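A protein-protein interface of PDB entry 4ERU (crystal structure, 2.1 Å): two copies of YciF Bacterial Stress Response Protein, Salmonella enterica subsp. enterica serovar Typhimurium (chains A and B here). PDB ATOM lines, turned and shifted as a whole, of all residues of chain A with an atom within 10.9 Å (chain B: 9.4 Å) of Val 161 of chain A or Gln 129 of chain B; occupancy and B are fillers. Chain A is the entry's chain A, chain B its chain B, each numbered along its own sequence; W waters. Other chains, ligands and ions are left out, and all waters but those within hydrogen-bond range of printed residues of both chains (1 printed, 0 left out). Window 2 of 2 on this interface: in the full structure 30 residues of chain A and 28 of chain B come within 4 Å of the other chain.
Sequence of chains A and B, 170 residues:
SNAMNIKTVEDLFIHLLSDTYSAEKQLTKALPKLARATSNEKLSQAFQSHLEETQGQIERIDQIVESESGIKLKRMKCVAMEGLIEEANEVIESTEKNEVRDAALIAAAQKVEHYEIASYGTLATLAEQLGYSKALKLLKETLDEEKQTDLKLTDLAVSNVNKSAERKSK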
ATOM      1  N   ASN A  40      34.374  17.369  25.762  1.00  0.00           N
ATOM      2  CA  ASN A  40      33.118  17.867  25.210  1.00  0.00           C
ATOM      3  C   ASN A  40      32.835  19.263  25.714  1.00  0.00           C
ATOM      4  O   ASN A  40      32.691  19.477  26.920  1.00  0.00           O
ATOM      5  CB  ASN A  40      31.933  16.981  25.557  1.00  0.00           C
ATOM      6  CG  ASN A  40      30.665  17.446  24.865  1.00  0.00           C
ATOM      7  OD1 ASN A  40      29.843  18.141  25.446  1.00  0.00           O
ATOM      8  ND2 ASN A  40      30.535  17.104  23.583  1.00  0.00           N
ATOM      9  N   LYS A  42      30.147  21.334  25.403  1.00  0.00           N
ATOM     10  CA  LYS A  42      28.855  21.485  26.069  1.00  0.00           C
ATOM     11  C   LYS A  42      28.841  21.009  27.541  1.00  0.00           C
ATOM     12  O   LYS A  42      28.235  21.662  28.401  1.00  0.00           O
ATOM     13  CB  LYS A  42      27.738  20.792  25.283  1.00  0.00           C
ATOM     14  CG  LYS A  42      27.060  21.667  24.227  1.00  0.00           C
ATOM     15  CD  LYS A  42      25.790  20.996  23.699  1.00  0.00           C
ATOM     16  CE  LYS A  42      26.111  19.755  22.848  1.00  0.00           C
ATOM     17  NZ  LYS A  42      25.172  18.613  23.119  1.00  0.00           N
ATOM     18  N   ASN A  98      37.681  11.130  26.700  1.00  0.00           N
ATOM     19  CA  ASN A  98      36.797  10.920  25.564  1.00  0.00           C
ATOM     20  C   ASN A  98      35.333  10.811  26.017  1.00  0.00           C
ATOM     21  O   ASN A  98      34.994  11.123  27.186  1.00  0.00           O
ATOM     22  CB  ASN A  98      37.226   9.664  24.794  1.00  0.00           C
ATOM     23  CG  ASN A  98      37.224   8.413  25.668  1.00  0.00           C
ATOM     24  OD1 ASN A  98      36.557   8.356  26.716  1.00  0.00           O
ATOM     25  ND2 ASN A  98      37.980   7.400  25.242  1.00  0.00           N
ATOM     26  N   GLU A  99      34.478  10.366  25.101  1.00  0.00           N
ATOM     27  CA  GLU A  99      33.049  10.264  25.358  1.00  0.00           C
ATOM     28  C   GLU A  99      32.700   9.288  26.478  1.00  0.00           C
ATOM     29  O   GLU A  99      31.662   9.435  27.105  1.00  0.00           O
ATOM     30  CB  GLU A  99      32.258   9.950  24.069  1.00  0.00           C
ATOM     31  CG  GLU A  99      32.579   8.608  23.424  1.00  0.00           C
ATOM     32  CD  GLU A  99      33.987   8.558  22.758  1.00  0.00           C
ATOM     33  OE1 GLU A  99      34.518   7.430  22.614  1.00  0.00           O
ATOM     34  OE2 GLU A  99      34.567   9.623  22.391  1.00  0.00           O
ATOM     35  N   VAL A 100      33.566   8.316  26.733  1.00  0.00           N
ATOM     36  CA  VAL A 100      33.343   7.344  27.786  1.00  0.00           C
ATOM     37  C   VAL A 100      33.567   8.033  29.132  1.00  0.00           C
ATOM     38  O   VAL A 100      32.784   7.872  30.069  1.00  0.00           O
ATOM     39  CB  VAL A 100      34.274   6.094  27.648  1.00  0.00           C
ATOM     40  CG1 VAL A 100      34.041   5.100  28.804  1.00  0.00           C
ATOM     41  CG2 VAL A 100      34.074   5.386  26.261  1.00  0.00           C
ATOM     42  N   ARG A 101      34.640   8.813  29.220  1.00  0.00           N
ATOM     43  CA  ARG A 101      34.819   9.639  30.395  1.00  0.00           C
ATOM     44  C   ARG A 101      33.607  10.562  30.569  1.00  0.00           C
ATOM     45  O   ARG A 101      33.054  10.681  31.670  1.00  0.00           O
ATOM     46  CB  ARG A 101      36.120  10.460  30.338  1.00  0.00           C
ATOM     47  CG  ARG A 101      36.315  11.252  31.648  1.00  0.00           C
ATOM     48  CD  ARG A 101      37.438  12.255  31.569  1.00  0.00           C
ATOM     49  NE  ARG A 101      38.712  11.563  31.578  1.00  0.00           N
ATOM     50  CZ  ARG A 101      39.896  12.154  31.480  1.00  0.00           C
ATOM     51  NH1 ARG A 101      40.010  13.474  31.324  1.00  0.00           N
ATOM     52  NH2 ARG A 101      40.964  11.398  31.523  1.00  0.00           N
ATOM     53  N   ASP A 102      33.167  11.191  29.486  1.00  0.00           N
ATOM     54  CA  ASP A 102      32.052  12.123  29.602  1.00  0.00           C
ATOM     55  C   ASP A 102      30.819  11.444  30.228  1.00  0.00           C
ATOM     56  O   ASP A 102      30.227  11.978  31.170  1.00  0.00           O
ATOM     57  CB  ASP A 102      31.681  12.729  28.257  1.00  0.00           C
ATOM     58  CG  ASP A 102      32.758  13.675  27.733  1.00  0.00           C
ATOM     59  OD1 ASP A 102      33.674  14.054  28.500  1.00  0.00           O
ATOM     60  OD2 ASP A 102      32.716  14.002  26.532  1.00  0.00           O
ATOM     61  N   ALA A 103      30.458  10.284  29.691  1.00  0.00           N
ATOM     62  CA  ALA A 103      29.338   9.492  30.219  1.00  0.00           C
ATOM     63  C   ALA A 103      29.493   9.250  31.712  1.00  0.00           C
ATOM     64  O   ALA A 103      28.530   9.359  32.466  1.00  0.00           O
ATOM     65  CB  ALA A 103      29.217   8.156  29.466  1.00  0.00           C
ATOM     66  N   ALA A 104      30.706   8.925  32.136  1.00  0.00           N
ATOM     67  CA  ALA A 104      30.964   8.522  33.512  1.00  0.00           C
ATOM     68  C   ALA A 104      31.010   9.714  34.452  1.00  0.00           C
ATOM     69  O   ALA A 104      30.588   9.618  35.613  1.00  0.00           O
ATOM     70  CB  ALA A 104      32.269   7.699  33.585  1.00  0.00           C
ATOM     71  N   ILE A 106      29.211  12.556  33.814  1.00  0.00           N
ATOM     72  CA  ILE A 106      27.805  12.945  33.917  1.00  0.00           C
ATOM     73  C   ILE A 106      27.119  12.118  34.985  1.00  0.00           C
ATOM     74  O   ILE A 106      26.446  12.681  35.849  1.00  0.00           O
ATOM     75  CB  ILE A 106      27.066  12.812  32.585  1.00  0.00           C
ATOM     76  CG1 ILE A 106      27.541  13.900  31.619  1.00  0.00           C
ATOM     77  CG2 ILE A 106      25.548  13.021  32.802  1.00  0.00           C
ATOM     78  CD1 ILE A 106      27.228  13.569  30.150  1.00  0.00           C
ATOM     79  N   ALA A 107      27.357  10.810  34.977  1.00  0.00           N
ATOM     80  CA  ALA A 107      26.785   9.931  35.995  1.00  0.00           C
ATOM     81  C   ALA A 107      27.180  10.342  37.423  1.00  0.00           C
ATOM     82  O   ALA A 107      26.334  10.389  38.328  1.00  0.00           O
ATOM     83  CB  ALA A 107      27.167   8.457  35.712  1.00  0.00           C
ATOM     84  N   LEU A 153      21.722  17.655  32.825  1.00  0.00           N
ATOM     85  CA  LEU A 153      22.740  16.596  32.772  1.00  0.00           C
ATOM     86  C   LEU A 153      22.178  15.336  32.097  1.00  0.00           C
ATOM     87  O   LEU A 153      22.888  14.679  31.378  1.00  0.00           O
ATOM     88  CB  LEU A 153      23.263  16.260  34.173  1.00  0.00           C
ATOM     89  CG  LEU A 153      24.225  17.307  34.779  1.00  0.00           C
ATOM     90  CD1 LEU A 153      24.389  17.145  36.279  1.00  0.00           C
ATOM     91  CD2 LEU A 153      25.614  17.298  34.087  1.00  0.00           C
ATOM     92  N   THR A 154      20.909  15.015  32.343  1.00  0.00           N
ATOM     93  CA  THR A 154      20.257  13.919  31.617  1.00  0.00           C
ATOM     94  C   THR A 154      20.255  14.174  30.095  1.00  0.00           C
ATOM     95  O   THR A 154      20.616  13.283  29.298  1.00  0.00           O
ATOM     96  CB  THR A 154      18.848  13.630  32.167  1.00  0.00           C
ATOM     97  OG1 THR A 154      18.965  13.090  33.493  1.00  0.00           O
ATOM     98  CG2 THR A 154      18.085  12.634  31.289  1.00  0.00           C
ATOM     99  N   ASP A 155      19.883  15.395  29.694  1.00  0.00           N
ATOM    100  CA  ASP A 155      19.989  15.809  28.293  1.00  0.00           C
ATOM    101  C   ASP A 155      21.362  15.523  27.708  1.00  0.00           C
ATOM    102  O   ASP A 155      21.456  14.884  26.641  1.00  0.00           O
ATOM    103  CB  ASP A 155      19.629  17.291  28.110  1.00  0.00           C
ATOM    104  CG  ASP A 155      18.153  17.485  27.786  1.00  0.00           C
ATOM    105  OD1 ASP A 155      17.380  16.489  27.808  1.00  0.00           O
ATOM    106  OD2 ASP A 155      17.758  18.633  27.515  1.00  0.00           O
ATOM    107  N   LEU A 156      22.424  15.943  28.408  1.00  0.00           N
ATOM    108  CA  LEU A 156      23.788  15.620  27.971  1.00  0.00           C
ATOM    109  C   LEU A 156      24.094  14.116  27.978  1.00  0.00           C
ATOM    110  O   LEU A 156      24.763  13.635  27.062  1.00  0.00           O
ATOM    111  CB  LEU A 156      24.847  16.405  28.759  1.00  0.00           C
ATOM    112  CG  LEU A 156      24.804  17.933  28.563  1.00  0.00           C
ATOM    113  CD1 LEU A 156      25.718  18.592  29.558  1.00  0.00           C
ATOM    114  CD2 LEU A 156      25.182  18.345  27.157  1.00  0.00           C
ATOM    115  N   ALA A 157      23.606  13.370  28.975  1.00  0.00           N
ATOM    116  CA  ALA A 157      23.837  11.898  29.010  1.00  0.00           C
ATOM    117  C   ALA A 157      23.285  11.211  27.742  1.00  0.00           C
ATOM    118  O   ALA A 157      23.942  10.352  27.118  1.00  0.00           O
ATOM    119  CB  ALA A 157      23.196  11.256  30.271  1.00  0.00           C
ATOM    120  N   VAL A 158      22.053  11.582  27.400  1.00  0.00           N
ATOM    121  CA  VAL A 158      21.341  11.042  26.248  1.00  0.00           C
ATOM    122  C   VAL A 158      21.944  11.540  24.917  1.00  0.00           C
ATOM    123  O   VAL A 158      22.050  10.790  23.967  1.00  0.00           O
ATOM    124  CB  VAL A 158      19.819  11.353  26.358  1.00  0.00           C
ATOM    125  CG1 VAL A 158      19.112  11.028  25.067  1.00  0.00           C
ATOM    126  CG2 VAL A 158      19.204  10.569  27.526  1.00  0.00           C
ATOM    127  N   SER A 159      22.355  12.798  24.883  1.00  0.00           N
ATOM    128  CA  SER A 159      23.071  13.404  23.763  1.00  0.00           C
ATOM    129  C   SER A 159      24.511  12.887  23.524  1.00  0.00           C
ATOM    130  O   SER A 159      25.107  13.179  22.483  1.00  0.00           O
ATOM    131  CB  SER A 159      23.130  14.904  24.012  1.00  0.00           C
ATOM    132  OG  SER A 159      23.714  15.591  22.931  1.00  0.00           O
ATOM    133  N   ASN A 160      25.077  12.147  24.479  1.00  0.00           N
ATOM    134  CA  ASN A 160      26.429  11.545  24.356  1.00  0.00           C
ATOM    135  C   ASN A 160      26.458  10.351  23.373  1.00  0.00           C
ATOM    136  O   ASN A 160      27.542   9.884  23.014  1.00  0.00           O
ATOM    137  CB  ASN A 160      26.935  11.092  25.756  1.00  0.00           C
ATOM    138  CG  ASN A 160      28.479  11.137  25.912  1.00  0.00           C
ATOM    139  OD1 ASN A 160      29.134  12.121  25.577  1.00  0.00           O
ATOM    140  ND2 ASN A 160      29.042  10.075  26.468  1.00  0.00           N
ATOM    141  N   VAL A 161      25.284   9.870  22.933  1.00  0.00           N
ATOM    142  CA  VAL A 161      25.168   8.750  21.951  1.00  0.00           C
ATOM    143  C   VAL A 161      25.788   9.019  20.551  1.00  0.00           C
ATOM    144  O   VAL A 161      26.642   9.903  20.353  1.00  0.00           O
ATOM    145  CB  VAL A 161      23.678   8.287  21.746  1.00  0.00           C
ATOM    146  CG1 VAL A 161      23.578   7.170  20.682  1.00  0.00           C
ATOM    147  CG2 VAL A 161      23.018   7.844  23.055  1.00  0.00           C
ATOM    148  N   THR B   8      35.148   1.356  27.517  1.00  0.00           N
ATOM    149  CA  THR B   8      34.020   1.438  26.605  1.00  0.00           C
ATOM    150  C   THR B   8      32.732   1.738  27.378  1.00  0.00           C
ATOM    151  O   THR B   8      32.669   1.545  28.606  1.00  0.00           O
ATOM    152  CB  THR B   8      33.816   0.100  25.826  1.00  0.00           C
ATOM    153  OG1 THR B   8      33.509  -0.949  26.745  1.00  0.00           O
ATOM    154  CG2 THR B   8      35.082  -0.304  24.977  1.00  0.00           C
ATOM    155  N   VAL B   9      31.712   2.187  26.653  1.00  0.00           N
ATOM    156  CA  VAL B   9      30.393   2.349  27.224  1.00  0.00           C
ATOM    157  C   VAL B   9      29.903   1.034  27.854  1.00  0.00           C
ATOM    158  O   VAL B   9      29.279   1.046  28.943  1.00  0.00           O
ATOM    159  CB  VAL B   9      29.389   2.902  26.199  1.00  0.00           C
ATOM    160  CG1 VAL B   9      27.961   2.996  26.831  1.00  0.00           C
ATOM    161  CG2 VAL B   9      29.861   4.271  25.701  1.00  0.00           C
ATOM    162  N   GLU B  10      30.186  -0.094  27.210  1.00  0.00           N
ATOM    163  CA  GLU B  10      29.793  -1.397  27.767  1.00  0.00           C
ATOM    164  C   GLU B  10      30.475  -1.655  29.122  1.00  0.00           C
ATOM    165  O   GLU B  10      29.842  -2.150  30.052  1.00  0.00           O
ATOM    166  CB  GLU B  10      30.091  -2.533  26.770  1.00  0.00           C
ATOM    167  CG  GLU B  10      29.026  -3.635  26.712  1.00  0.00           C
ATOM    168  CD  GLU B  10      29.547  -5.031  27.093  1.00  0.00           C
ATOM    169  OE1 GLU B  10      30.675  -5.388  26.656  1.00  0.00           O
ATOM    170  OE2 GLU B  10      28.812  -5.794  27.787  1.00  0.00           O
ATOM    171  N   LEU B  12      31.449   0.659  31.213  1.00  0.00           N
ATOM    172  CA  LEU B  12      30.852   1.596  32.160  1.00  0.00           C
ATOM    173  C   LEU B  12      29.530   1.027  32.663  1.00  0.00           C
ATOM    174  O   LEU B  12      29.268   1.073  33.892  1.00  0.00           O
ATOM    175  CB  LEU B  12      30.607   2.960  31.532  1.00  0.00           C
ATOM    176  CG  LEU B  12      29.954   4.018  32.433  1.00  0.00           C
ATOM    177  CD1 LEU B  12      30.786   4.282  33.659  1.00  0.00           C
ATOM    178  CD2 LEU B  12      29.747   5.341  31.645  1.00  0.00           C
ATOM    179  N   PHE B  13      28.718   0.496  31.731  1.00  0.00           N
ATOM    180  CA  PHE B  13      27.408  -0.081  32.118  1.00  0.00           C
ATOM    181  C   PHE B  13      27.591  -1.215  33.152  1.00  0.00           C
ATOM    182  O   PHE B  13      26.937  -1.263  34.199  1.00  0.00           O
ATOM    183  CB  PHE B  13      26.654  -0.576  30.891  1.00  0.00           C
ATOM    184  CG  PHE B  13      25.338  -1.225  31.206  1.00  0.00           C
ATOM    185  CD1 PHE B  13      24.214  -0.453  31.424  1.00  0.00           C
ATOM    186  CD2 PHE B  13      25.223  -2.624  31.291  1.00  0.00           C
ATOM    187  CE1 PHE B  13      22.971  -1.025  31.721  1.00  0.00           C
ATOM    188  CE2 PHE B  13      23.995  -3.203  31.576  1.00  0.00           C
ATOM    189  CZ  PHE B  13      22.856  -2.386  31.804  1.00  0.00           C
ATOM    190  N   GLY B 121      18.781   6.071  36.543  1.00  0.00           N
ATOM    191  CA  GLY B 121      18.540   6.958  35.406  1.00  0.00           C
ATOM    192  C   GLY B 121      19.675   6.769  34.440  1.00  0.00           C
ATOM    193  O   GLY B 121      19.460   6.648  33.236  1.00  0.00           O
ATOM    194  N   THR B 122      20.901   6.728  34.978  1.00  0.00           N
ATOM    195  CA  THR B 122      22.076   6.527  34.138  1.00  0.00           C
ATOM    196  C   THR B 122      22.045   5.147  33.493  1.00  0.00           C
ATOM    197  O   THR B 122      22.328   5.007  32.303  1.00  0.00           O
ATOM    198  CB  THR B 122      23.396   6.675  34.945  1.00  0.00           C
ATOM    199  OG1 THR B 122      23.524   8.024  35.330  1.00  0.00           O
ATOM    200  CG2 THR B 122      24.607   6.335  34.045  1.00  0.00           C
ATOM    201  N   LEU B 123      21.734   4.121  34.292  1.00  0.00           N
ATOM    202  CA  LEU B 123      21.668   2.750  33.734  1.00  0.00           C
ATOM    203  C   LEU B 123      20.676   2.620  32.547  1.00  0.00           C
ATOM    204  O   LEU B 123      21.006   1.998  31.550  1.00  0.00           O
ATOM    205  CB  LEU B 123      21.383   1.720  34.821  1.00  0.00           C
ATOM    206  CG  LEU B 123      22.603   1.532  35.761  1.00  0.00           C
ATOM    207  CD1 LEU B 123      22.156   0.747  37.003  1.00  0.00           C
ATOM    208  CD2 LEU B 123      23.830   0.854  35.076  1.00  0.00           C
ATOM    209  N   ALA B 124      19.495   3.226  32.660  1.00  0.00           N
ATOM    210  CA  ALA B 124      18.495   3.225  31.569  1.00  0.00           C
ATOM    211  C   ALA B 124      19.017   3.940  30.312  1.00  0.00           C
ATOM    212  O   ALA B 124      18.919   3.397  29.219  1.00  0.00           O
ATOM    213  CB  ALA B 124      17.202   3.858  32.015  1.00  0.00           C
ATOM    214  N   THR B 125      19.597   5.128  30.472  1.00  0.00           N
ATOM    215  CA  THR B 125      20.213   5.825  29.353  1.00  0.00           C
ATOM    216  C   THR B 125      21.239   4.925  28.597  1.00  0.00           C
ATOM    217  O   THR B 125      21.206   4.824  27.343  1.00  0.00           O
ATOM    218  CB  THR B 125      20.885   7.099  29.838  1.00  0.00           C
ATOM    219  OG1 THR B 125      19.886   8.022  30.293  1.00  0.00           O
ATOM    220  CG2 THR B 125      21.720   7.731  28.729  1.00  0.00           C
ATOM    221  N   LEU B 126      22.148   4.305  29.364  1.00  0.00           N
ATOM    222  CA  LEU B 126      23.192   3.456  28.815  1.00  0.00           C
ATOM    223  C   LEU B 126      22.634   2.180  28.169  1.00  0.00           C
ATOM    224  O   LEU B 126      23.045   1.813  27.085  1.00  0.00           O
ATOM    225  CB  LEU B 126      24.225   3.107  29.896  1.00  0.00           C
ATOM    226  CG  LEU B 126      25.048   4.270  30.464  1.00  0.00           C
ATOM    227  CD1 LEU B 126      26.045   3.757  31.509  1.00  0.00           C
ATOM    228  CD2 LEU B 126      25.757   5.059  29.393  1.00  0.00           C
ATOM    229  N   ALA B 127      21.702   1.504  28.853  1.00  0.00           N
ATOM    230  CA  ALA B 127      21.003   0.352  28.275  1.00  0.00           C
ATOM    231  C   ALA B 127      20.385   0.678  26.918  1.00  0.00           C
ATOM    232  O   ALA B 127      20.561  -0.078  25.940  1.00  0.00           O
ATOM    233  CB  ALA B 127      19.938  -0.211  29.246  1.00  0.00           C
ATOM    234  N   GLU B 128      19.652   1.785  26.855  1.00  0.00           N
ATOM    235  CA  GLU B 128      19.092   2.190  25.586  1.00  0.00           C
ATOM    236  C   GLU B 128      20.202   2.369  24.546  1.00  0.00           C
ATOM    237  O   GLU B 128      20.105   1.835  23.444  1.00  0.00           O
ATOM    238  CB  GLU B 128      18.254   3.455  25.697  1.00  0.00           C
ATOM    239  CG  GLU B 128      17.680   3.792  24.342  1.00  0.00           C
ATOM    240  CD  GLU B 128      16.592   4.824  24.372  1.00  0.00           C
ATOM    241  OE1 GLU B 128      16.375   5.467  25.422  1.00  0.00           O
ATOM    242  OE2 GLU B 128      15.946   4.994  23.319  1.00  0.00           O
ATOM    243  N   GLN B 129      21.270   3.083  24.911  1.00  0.00           N
ATOM    244  CA  GLN B 129      22.377   3.297  23.996  1.00  0.00           C
ATOM    245  C   GLN B 129      23.010   1.989  23.492  1.00  0.00           C
ATOM    246  O   GLN B 129      23.445   1.900  22.332  1.00  0.00           O
ATOM    247  CB  GLN B 129      23.447   4.166  24.656  1.00  0.00           C
ATOM    248  CG  GLN B 129      24.672   4.396  23.761  1.00  0.00           C
ATOM    249  CD  GLN B 129      25.665   5.382  24.342  1.00  0.00           C
ATOM    250  OE1 GLN B 129      26.813   5.447  23.889  1.00  0.00           O
ATOM    251  NE2 GLN B 129      25.223   6.182  25.313  1.00  0.00           N
ATOM    252  N   LEU B 130      23.081   0.994  24.375  1.00  0.00           N
ATOM    253  CA  LEU B 130      23.713  -0.275  24.057  1.00  0.00           C
ATOM    254  C   LEU B 130      22.778  -1.263  23.339  1.00  0.00           C
ATOM    255  O   LEU B 130      23.221  -2.339  22.929  1.00  0.00           O
ATOM    256  CB  LEU B 130      24.314  -0.917  25.331  1.00  0.00           C
ATOM    257  CG  LEU B 130      25.547  -0.163  25.881  1.00  0.00           C
ATOM    258  CD1 LEU B 130      25.902  -0.586  27.304  1.00  0.00           C
ATOM    259  CD2 LEU B 130      26.763  -0.373  24.958  1.00  0.00           C
ATOM    260  N   GLY B 131      21.505  -0.896  23.183  1.00  0.00           N
ATOM    261  CA  GLY B 131      20.545  -1.751  22.512  1.00  0.00           C
ATOM    262  C   GLY B 131      20.014  -2.868  23.398  1.00  0.00           C
ATOM    263  O   GLY B 131      19.477  -3.847  22.880  1.00  0.00           O
ATOM    264  N   TYR B 132      20.126  -2.713  24.725  1.00  0.00           N
ATOM    265  CA  TYR B 132      19.649  -3.742  25.678  1.00  0.00           C
ATOM    266  C   TYR B 132      18.174  -3.525  26.001  1.00  0.00           C
ATOM    267  O   TYR B 132      17.825  -2.902  27.011  1.00  0.00           O
ATOM    268  CB  TYR B 132      20.478  -3.773  26.976  1.00  0.00           C
ATOM    269  CG  TYR B 132      21.982  -4.004  26.849  1.00  0.00           C
ATOM    270  CD1 TYR B 132      22.538  -4.695  25.766  1.00  0.00           C
ATOM    271  CD2 TYR B 132      22.851  -3.571  27.848  1.00  0.00           C
ATOM    272  CE1 TYR B 132      23.937  -4.918  25.667  1.00  0.00           C
ATOM    273  CE2 TYR B 132      24.239  -3.791  27.762  1.00  0.00           C
ATOM    274  CZ  TYR B 132      24.772  -4.462  26.674  1.00  0.00           C
ATOM    275  OH  TYR B 132      26.136  -4.691  26.604  1.00  0.00           O
ATOM    276  N   SER B 133      17.306  -4.061  25.152  1.00  0.00           N
ATOM    277  CA  SER B 133      15.885  -3.715  25.195  1.00  0.00           C
ATOM    278  C   SER B 133      15.153  -4.213  26.421  1.00  0.00           C
ATOM    279  O   SER B 133      14.378  -3.475  27.007  1.00  0.00           O
ATOM    280  CB  SER B 133      15.164  -4.206  23.914  1.00  0.00           C
ATOM    281  OG  SER B 133      15.579  -3.404  22.820  1.00  0.00           O
ATOM    282  N   LEU B 136      16.498  -2.305  29.491  1.00  0.00           N
ATOM    283  CA  LEU B 136      15.917  -0.964  29.546  1.00  0.00           C
ATOM    284  C   LEU B 136      14.538  -0.989  30.179  1.00  0.00           C
ATOM    285  O   LEU B 136      14.249  -0.200  31.056  1.00  0.00           O
ATOM    286  CB  LEU B 136      15.848  -0.328  28.156  1.00  0.00           C
ATOM    287  CG  LEU B 136      15.146   1.024  27.989  1.00  0.00           C
ATOM    288  CD1 LEU B 136      15.781   2.200  28.812  1.00  0.00           C
ATOM    289  CD2 LEU B 136      15.045   1.407  26.480  1.00  0.00           C
ATOM    290  N   LEU B 139      14.954  -1.707  33.980  1.00  0.00           N
ATOM    291  CA  LEU B 139      15.575  -0.584  34.684  1.00  0.00           C
ATOM    292  C   LEU B 139      14.613   0.564  34.892  1.00  0.00           C
ATOM    293  O   LEU B 139      14.612   1.203  35.945  1.00  0.00           O
ATOM    294  CB  LEU B 139      16.812  -0.095  33.931  1.00  0.00           C
ATOM    295  CG  LEU B 139      17.988  -1.087  33.995  1.00  0.00           C
ATOM    296  CD1 LEU B 139      18.905  -0.839  32.789  1.00  0.00           C
ATOM    297  CD2 LEU B 139      18.788  -1.094  35.322  1.00  0.00           C
HETATM  298  O   HOH W   1      24.170   8.589  38.100  1.00  0.00           O
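OG1 of Thr 8 of chain B lies close to N of Glu 10 of chain B, at 3.5 Å.
OD1 of Asn 98 of chain A sits at hydrogen-bond distance from N of Val 100 of chain A (3.0 Å).
The side-chain hydroxyl (OG1) of Thr 125 of chain B is in hydrogen-bond range of the backbone carbonyl oxygen (O) of Gly 121 of chain B (3.3 Å).
Among the printed residues, pairs that only touch across the chains: Val 100 of chain A with Thr 8 of chain B, Val 100 of chain A with Val 9 of chain B, Ala 103 of chain A with Leu 12 of chain B, Ala 104 of chain A with Leu 12 of chain B, Ala 107 of chain A with Thr 122 of chain B, Ala 157 of chain A with Thr 125 of chain B, Val 158 of chain A with Thr 125 of chain B and Val 161 of chain A with Gln 129 of chain B.
Of the printed residues of chain B, Ala 104 of chain A touches Leu 12 (3.7 Å).
Of the printed residues of chain B, Ala 107 of chain A touches Thr 122 (3.7 Å).
Val 161 of chain A touches just one residue of chain B: Gln 129 (3.6 Å).
Of the printed residues of chain A, Thr 8 of chain B touches Val 100 (3.8 Å).
Printed residues of chain A within 4 Å of Val 9 of chain B: Val 100.
Of the printed residues of chain A, Thr 125 of chain B touches Ala 157 (3.8 Å) and Val 158 (3.8 Å).
No residue of chain A comes within 4 Å of Leu 126 of chain B.
No residue of chain A comes within 4 Å of Ala 127 of chain B.
No residue of chain A comes within 4 Å of Leu 130 of chain B.
No residue of chain A comes within 4 Å of Gly 131 of chain B.
The nearest residue of chain B that does not touch Val 161 of chain A is Thr 125 of chain B (5.5 Å).
The nearest residue of chain A that does not touch Gln 129 of chain B is Asn 160 of chain A (4.6 Å).
The nearest printed residue of chain A that does not touch Leu 12 of chain B is Val 100 of chain A (4.3 Å).
Printed residues of chain A that touch a printed residue of chain B: Val 100, Ala 103, Ala 104, Ala 107, Ala 157, Val 158 and Val 161.
Hydrophobic or aromatic side chains of chain A within 4 Å of the printed part of chain B: Val 100, Ala 103, Ala 104, Ala 107, Val 158 and Val 161.
Of the 20 printed residues of chain B, 6 touch a printed residue of chain A.
Among the printed residues, no Asp or Glu carboxylate lies within 4 Å of a Lys or Arg side-chain nitrogen of the other chain.
No position is printed for both chains.
Of the 8 pairs that touch across the chains among the printed residues, none has its exchanged pair printed and touching as well.
Water W1 bridges the backbone carbonyl oxygen (O) of Ala 107 of chain A (2.8 Å) and the side-chain hydroxyl (OG1) of Thr 122 of chain B (2.9 Å).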
